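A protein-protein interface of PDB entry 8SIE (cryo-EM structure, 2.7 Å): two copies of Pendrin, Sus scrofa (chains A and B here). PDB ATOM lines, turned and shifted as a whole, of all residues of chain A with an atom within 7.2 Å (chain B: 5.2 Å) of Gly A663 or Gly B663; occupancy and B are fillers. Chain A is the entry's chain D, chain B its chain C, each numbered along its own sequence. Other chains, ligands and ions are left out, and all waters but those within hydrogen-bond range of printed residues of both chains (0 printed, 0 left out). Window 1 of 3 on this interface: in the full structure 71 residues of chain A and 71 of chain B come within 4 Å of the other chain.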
ATOM      1  N   ARG A 549      13.121  17.855 -20.688  1.00  0.00           N
ATOM      2  CA  ARG A 549      12.519  16.542 -20.514  1.00  0.00           C
ATOM      3  C   ARG A 549      11.379  16.390 -21.511  1.00  0.00           C
ATOM      4  O   ARG A 549      10.435  17.188 -21.506  1.00  0.00           O
ATOM      5  CB  ARG A 549      12.011  16.342 -19.088  1.00  0.00           C
ATOM      6  CG  ARG A 549      11.742  14.886 -18.755  1.00  0.00           C
ATOM      7  CD  ARG A 549      11.082  14.721 -17.404  1.00  0.00           C
ATOM      8  NE  ARG A 549      10.151  13.599 -17.399  1.00  0.00           N
ATOM      9  CZ  ARG A 549      10.494  12.339 -17.161  1.00  0.00           C
ATOM     10  NH1 ARG A 549      11.748  11.998 -16.916  1.00  0.00           N
ATOM     11  NH2 ARG A 549       9.555  11.399 -17.172  1.00  0.00           N
ATOM     12  N   PHE A 550      11.478  15.368 -22.360  1.00  0.00           N
ATOM     13  CA  PHE A 550      10.468  15.025 -23.356  1.00  0.00           C
ATOM     14  C   PHE A 550       9.903  13.664 -22.970  1.00  0.00           C
ATOM     15  O   PHE A 550      10.537  12.632 -23.213  1.00  0.00           O
ATOM     16  CB  PHE A 550      11.082  15.006 -24.753  1.00  0.00           C
ATOM     17  CG  PHE A 550      10.078  14.998 -25.870  1.00  0.00           C
ATOM     18  CD1 PHE A 550       9.376  16.145 -26.198  1.00  0.00           C
ATOM     19  CD2 PHE A 550       9.854  13.849 -26.607  1.00  0.00           C
ATOM     20  CE1 PHE A 550       8.459  16.137 -27.231  1.00  0.00           C
ATOM     21  CE2 PHE A 550       8.940  13.837 -27.640  1.00  0.00           C
ATOM     22  CZ  PHE A 550       8.243  14.982 -27.953  1.00  0.00           C
ATOM     23  N   SER A 551       8.713  13.660 -22.370  1.00  0.00           N
ATOM     24  CA  SER A 551       8.184  12.466 -21.707  1.00  0.00           C
ATOM     25  C   SER A 551       7.321  11.652 -22.672  1.00  0.00           C
ATOM     26  O   SER A 551       6.095  11.592 -22.566  1.00  0.00           O
ATOM     27  CB  SER A 551       7.402  12.861 -20.461  1.00  0.00           C
ATOM     28  OG  SER A 551       8.202  13.615 -19.570  1.00  0.00           O
ATOM     29  N   SER A 552       7.995  10.999 -23.611  1.00  0.00           N
ATOM     30  CA  SER A 552       7.341  10.139 -24.588  1.00  0.00           C
ATOM     31  C   SER A 552       8.417   9.434 -25.405  1.00  0.00           C
ATOM     32  O   SER A 552       9.533   9.942 -25.527  1.00  0.00           O
ATOM     33  CB  SER A 552       6.416  10.942 -25.515  1.00  0.00           C
ATOM     34  OG  SER A 552       5.703  10.104 -26.405  1.00  0.00           O
ATOM     35  N   LEU A 660      19.351  16.490 -22.461  1.00  0.00           N
ATOM     36  CA  LEU A 660      18.049  15.924 -22.795  1.00  0.00           C
ATOM     37  C   LEU A 660      17.744  14.797 -21.816  1.00  0.00           C
ATOM     38  O   LEU A 660      18.370  13.735 -21.868  1.00  0.00           O
ATOM     39  CB  LEU A 660      18.029  15.418 -24.235  1.00  0.00           C
ATOM     40  CG  LEU A 660      18.046  16.472 -25.344  1.00  0.00           C
ATOM     41  CD1 LEU A 660      17.939  15.813 -26.705  1.00  0.00           C
ATOM     42  CD2 LEU A 660      16.926  17.477 -25.148  1.00  0.00           C
ATOM     43  N   ASP A 661      16.781  15.028 -20.925  1.00  0.00           N
ATOM     44  CA  ASP A 661      16.344  14.007 -19.979  1.00  0.00           C
ATOM     45  C   ASP A 661      15.447  13.021 -20.717  1.00  0.00           C
ATOM     46  O   ASP A 661      14.312  13.350 -21.076  1.00  0.00           O
ATOM     47  CB  ASP A 661      15.619  14.648 -18.800  1.00  0.00           C
ATOM     48  CG  ASP A 661      15.130  13.630 -17.787  1.00  0.00           C
ATOM     49  OD1 ASP A 661      15.585  12.467 -17.830  1.00  0.00           O
ATOM     50  OD2 ASP A 661      14.290  13.994 -16.940  1.00  0.00           O
ATOM     51  N   CYS A 662      15.952  11.812 -20.943  1.00  0.00           N
ATOM     52  CA  CYS A 662      15.276  10.807 -21.754  1.00  0.00           C
ATOM     53  C   CYS A 662      14.829   9.611 -20.917  1.00  0.00           C
ATOM     54  O   CYS A 662      14.886   8.465 -21.363  1.00  0.00           O
ATOM     55  CB  CYS A 662      16.179  10.347 -22.894  1.00  0.00           C
ATOM     56  SG  CYS A 662      16.878  11.680 -23.887  1.00  0.00           S
ATOM     57  N   GLY A 663      14.370   9.871 -19.692  1.00  0.00           N
ATOM     58  CA  GLY A 663      13.941   8.792 -18.821  1.00  0.00           C
ATOM     59  C   GLY A 663      12.599   8.196 -19.187  1.00  0.00           C
ATOM     60  O   GLY A 663      12.248   7.130 -18.673  1.00  0.00           O
ATOM     61  N   ALA A 664      11.843   8.855 -20.063  1.00  0.00           N
ATOM     62  CA  ALA A 664      10.524   8.386 -20.467  1.00  0.00           C
ATOM     63  C   ALA A 664      10.452   8.015 -21.943  1.00  0.00           C
ATOM     64  O   ALA A 664       9.351   7.833 -22.472  1.00  0.00           O
ATOM     65  CB  ALA A 664       9.467   9.441 -20.141  1.00  0.00           C
ATOM     66  N   VAL A 665      11.591   7.895 -22.623  1.00  0.00           N
ATOM     67  CA  VAL A 665      11.622   7.492 -24.028  1.00  0.00           C
ATOM     68  C   VAL A 665      11.495   5.972 -24.062  1.00  0.00           C
ATOM     69  O   VAL A 665      12.479   5.250 -23.900  1.00  0.00           O
ATOM     70  CB  VAL A 665      12.891   7.974 -24.735  1.00  0.00           C
ATOM     71  CG1 VAL A 665      12.896   7.524 -26.183  1.00  0.00           C
ATOM     72  CG2 VAL A 665      13.000   9.485 -24.650  1.00  0.00           C
ATOM     73  N   SER A 666      10.272   5.480 -24.270  1.00  0.00           N
ATOM     74  CA  SER A 666      10.017   4.046 -24.178  1.00  0.00           C
ATOM     75  C   SER A 666      10.643   3.288 -25.344  1.00  0.00           C
ATOM     76  O   SER A 666      11.299   2.260 -25.146  1.00  0.00           O
ATOM     77  CB  SER A 666       8.513   3.789 -24.112  1.00  0.00           C
ATOM     78  OG  SER A 666       7.902   4.607 -23.132  1.00  0.00           O
ATOM     79  N   ALA A 693      20.640  11.835 -20.827  1.00  0.00           N
ATOM     80  CA  ALA A 693      20.620  11.281 -19.484  1.00  0.00           C
ATOM     81  C   ALA A 693      19.405  10.384 -19.308  1.00  0.00           C
ATOM     82  O   ALA A 693      18.352  10.625 -19.906  1.00  0.00           O
ATOM     83  CB  ALA A 693      20.607  12.387 -18.430  1.00  0.00           C
ATOM     84  N   SER A 694      19.569   9.341 -18.494  1.00  0.00           N
ATOM     85  CA  SER A 694      18.506   8.427 -18.086  1.00  0.00           C
ATOM     86  C   SER A 694      17.947   7.596 -19.235  1.00  0.00           C
ATOM     87  O   SER A 694      16.830   7.082 -19.135  1.00  0.00           O
ATOM     88  CB  SER A 694      17.366   9.176 -17.386  1.00  0.00           C
ATOM     89  OG  SER A 694      17.776   9.658 -16.119  1.00  0.00           O
ATOM     90  N   LEU A 695      18.691   7.440 -20.326  1.00  0.00           N
ATOM     91  CA  LEU A 695      18.267   6.529 -21.380  1.00  0.00           C
ATOM     92  C   LEU A 695      18.365   5.084 -20.913  1.00  0.00           C
ATOM     93  O   LEU A 695      19.324   4.692 -20.244  1.00  0.00           O
ATOM     94  CB  LEU A 695      19.108   6.726 -22.640  1.00  0.00           C
ATOM     95  CG  LEU A 695      18.570   7.735 -23.650  1.00  0.00           C
ATOM     96  CD1 LEU A 695      19.587   7.998 -24.738  1.00  0.00           C
ATOM     97  CD2 LEU A 695      17.271   7.230 -24.249  1.00  0.00           C
ATOM     98  N   GLN A 696      17.364   4.290 -21.275  1.00  0.00           N
ATOM     99  CA  GLN A 696      17.324   2.892 -20.885  1.00  0.00           C
ATOM    100  C   GLN A 696      18.275   2.062 -21.742  1.00  0.00           C
ATOM    101  O   GLN A 696      18.729   2.486 -22.808  1.00  0.00           O
ATOM    102  CB  GLN A 696      15.903   2.346 -20.996  1.00  0.00           C
ATOM    103  CG  GLN A 696      15.005   2.720 -19.831  1.00  0.00           C
ATOM    104  CD  GLN A 696      15.469   2.112 -18.525  1.00  0.00           C
ATOM    105  OE1 GLN A 696      16.089   2.782 -17.700  1.00  0.00           O
ATOM    106  NE2 GLN A 696      15.165   0.835 -18.327  1.00  0.00           N
ATOM    107  N   VAL A 722      19.999  12.802 -14.475  1.00  0.00           N
ATOM    108  CA  VAL A 722      20.292  14.222 -14.608  1.00  0.00           C
ATOM    109  C   VAL A 722      20.761  14.714 -13.246  1.00  0.00           C
ATOM    110  O   VAL A 722      20.060  15.465 -12.559  1.00  0.00           O
ATOM    111  CB  VAL A 722      19.062  15.013 -15.093  1.00  0.00           C
ATOM    112  CG1 VAL A 722      19.427  16.467 -15.371  1.00  0.00           C
ATOM    113  CG2 VAL A 722      18.451  14.360 -16.316  1.00  0.00           C
ATOM    114  N   ARG B 549       9.985  -2.385 -13.064  1.00  0.00           N
ATOM    115  CA  ARG B 549       9.939  -1.247 -13.971  1.00  0.00           C
ATOM    116  C   ARG B 549       9.114  -1.626 -15.193  1.00  0.00           C
ATOM    117  O   ARG B 549       9.445  -2.591 -15.892  1.00  0.00           O
ATOM    118  CB  ARG B 549      11.340  -0.804 -14.388  1.00  0.00           C
ATOM    119  CG  ARG B 549      11.366   0.584 -14.996  1.00  0.00           C
ATOM    120  CD  ARG B 549      12.725   0.939 -15.557  1.00  0.00           C
ATOM    121  NE  ARG B 549      12.611   1.778 -16.743  1.00  0.00           N
ATOM    122  CZ  ARG B 549      12.497   3.099 -16.722  1.00  0.00           C
ATOM    123  NH1 ARG B 549      12.468   3.772 -15.583  1.00  0.00           N
ATOM    124  NH2 ARG B 549      12.411   3.762 -17.870  1.00  0.00           N
ATOM    125  N   ASP B 661       8.559   1.050 -10.306  1.00  0.00           N
ATOM    126  CA  ASP B 661       9.299   2.153 -10.910  1.00  0.00           C
ATOM    127  C   ASP B 661       8.495   2.679 -12.094  1.00  0.00           C
ATOM    128  O   ASP B 661       8.394   2.015 -13.131  1.00  0.00           O
ATOM    129  CB  ASP B 661      10.688   1.693 -11.339  1.00  0.00           C
ATOM    130  CG  ASP B 661      11.501   2.798 -11.985  1.00  0.00           C
ATOM    131  OD1 ASP B 661      11.124   3.982 -11.855  1.00  0.00           O
ATOM    132  OD2 ASP B 661      12.526   2.484 -12.622  1.00  0.00           O
ATOM    133  N   CYS B 662       7.927   3.871 -11.944  1.00  0.00           N
ATOM    134  CA  CYS B 662       7.016   4.448 -12.925  1.00  0.00           C
ATOM    135  C   CYS B 662       7.617   5.675 -13.601  1.00  0.00           C
ATOM    136  O   CYS B 662       6.922   6.651 -13.885  1.00  0.00           O
ATOM    137  CB  CYS B 662       5.683   4.800 -12.273  1.00  0.00           C
ATOM    138  SG  CYS B 662       4.924   3.459 -11.336  1.00  0.00           S
ATOM    139  N   GLY B 663       8.922   5.636 -13.873  1.00  0.00           N
ATOM    140  CA  GLY B 663       9.583   6.764 -14.502  1.00  0.00           C
ATOM    141  C   GLY B 663       9.255   6.939 -15.969  1.00  0.00           C
ATOM    142  O   GLY B 663       9.482   8.021 -16.517  1.00  0.00           O
ATOM    143  N   ALA B 664       8.730   5.900 -16.618  1.00  0.00           N
ATOM    144  CA  ALA B 664       8.416   5.946 -18.039  1.00  0.00           C
ATOM    145  C   ALA B 664       6.918   5.900 -18.321  1.00  0.00           C
ATOM    146  O   ALA B 664       6.523   5.687 -19.471  1.00  0.00           O
ATOM    147  CB  ALA B 664       9.120   4.803 -18.771  1.00  0.00           C
ATOM    148  N   VAL B 665       6.076   6.095 -17.307  1.00  0.00           N
ATOM    149  CA  VAL B 665       4.626   6.115 -17.496  1.00  0.00           C
ATOM    150  C   VAL B 665       4.260   7.503 -18.015  1.00  0.00           C
ATOM    151  O   VAL B 665       4.105   8.448 -17.243  1.00  0.00           O
ATOM    152  CB  VAL B 665       3.876   5.772 -16.207  1.00  0.00           C
ATOM    153  CG1 VAL B 665       2.378   5.821 -16.436  1.00  0.00           C
ATOM    154  CG2 VAL B 665       4.290   4.403 -15.704  1.00  0.00           C
ATOM    155  N   ALA B 693       7.344   4.956  -7.417  1.00  0.00           N
ATOM    156  CA  ALA B 693       8.512   5.821  -7.465  1.00  0.00           C
ATOM    157  C   ALA B 693       8.655   6.428  -8.852  1.00  0.00           C
ATOM    158  O   ALA B 693       8.293   5.804  -9.854  1.00  0.00           O
ATOM    159  CB  ALA B 693       9.782   5.055  -7.097  1.00  0.00           C
ATOM    160  N   SER B 694       9.174   7.656  -8.894  1.00  0.00           N
ATOM    161  CA  SER B 694       9.513   8.374 -10.119  1.00  0.00           C
ATOM    162  C   SER B 694       8.300   8.726 -10.972  1.00  0.00           C
ATOM    163  O   SER B 694       8.444   8.976 -12.171  1.00  0.00           O
ATOM    164  CB  SER B 694      10.529   7.591 -10.960  1.00  0.00           C
ATOM    165  OG  SER B 694      11.797   7.562 -10.332  1.00  0.00           O
ATOM    166  N   LEU B 695       7.105   8.760 -10.391  1.00  0.00           N
ATOM    167  CA  LEU B 695       5.944   9.243 -11.126  1.00  0.00           C
ATOM    168  C   LEU B 695       6.047  10.742 -11.368  1.00  0.00           C
ATOM    169  O   LEU B 695       6.458  11.504 -10.490  1.00  0.00           O
ATOM    170  CB  LEU B 695       4.653   8.925 -10.374  1.00  0.00           C
ATOM    171  CG  LEU B 695       3.992   7.592 -10.717  1.00  0.00           C
ATOM    172  CD1 LEU B 695       2.857   7.298  -9.764  1.00  0.00           C
ATOM    173  CD2 LEU B 695       3.492   7.614 -12.149  1.00  0.00           C
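Arg A549 touches Gly B663, and with the chains exchanged Gly A663 touches Arg B549.
Gly B663 touches its own counterpart, Gly A663.
Gly A663 touches Ala B664, and with the chains exchanged Ala A664 touches Gly B663.
Of the 6 pairs that touch across the chains among the printed residues, 5 have their exchanged pair printed and touching as well.
Of the printed residues of chain B, Arg A549 touches Gly B663 (3.4 Å).
Of the printed residues of chain B, Gly A663 touches Arg B549 (3.5 Å), Gly B663 (3.6 Å) and Ala B664 (3.9 Å).
Of the printed residues of chain B, Ala A664 touches Gly B663 (3.9 Å).
Printed residues of chain B within 4 Å of Gln A696: Arg B549.
Printed residues of chain A within 4 Å of Arg B549: Gly A663 and Gln A696.
Gly B663 touches just these residues of chain A: Arg A549, Gly A663 and Ala A664.
Of the printed residues of chain A, Ala B664 touches Gly A663 (3.9 Å).
The nearest residue of chain A that does not touch Gly B663 is Val A665 (6.5 Å).
The nearest printed residue of chain B that does not touch Gln A696 is Asp B661 (6.2 Å).
Hydrophobic or aromatic side chains of chain B within 4 Å of the printed part of chain A: Ala B664.
Of the 16 printed residues of chain A, 4 touch a printed residue of chain B.
Hydrophobic or aromatic side chains of chain A that line the printed part of chain B: Ala A664.
Among the printed residues, 6 pairs touch across the chains.
Among the printed residues, no Asp or Glu carboxylate lies within 4 Å of a Lys or Arg side-chain nitrogen of the other chain.
NE of Arg A549 is in hydrogen-bond range of OG of Ser A551.
The guanidinium group (NH1) of Arg A549 is in salt-bridge range of the side-chain carboxylate (OD2) of Asp A661, at 3.2 Å.
The side-chain carboxylate (OD1) of Asp A661 lies within hydrogen-bond range of the backbone NH (N) of Gly A663, at 3.4 Å.
NH1 of Arg B549 is in salt-bridge range of OD2 of Asp B661.
The side-chain carboxylate (OD1) of Asp B661 lies within hydrogen-bond range of the backbone NH (N) of Gly B663, 3.4 Å away.
O of Gly B663 sits at hydrogen-bond distance from NH2 of Arg A549 (3.4 Å).
The backbone carbonyl oxygen (O) of Gly A663 is in hydrogen-bond range of the guanidinium group (NH2) of Arg B549.
The side-chain amide nitrogen of Gln A696 sits close to the guanidinium group of Arg B549 (3.1 Å).
Among the printed residues, merely in contact across the chains: Gly A663 with Gly B663 (3.6 Å), Gly A663 with Ala B664 (3.9 Å) and Ala A664 with Gly B663 (3.9 Å).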
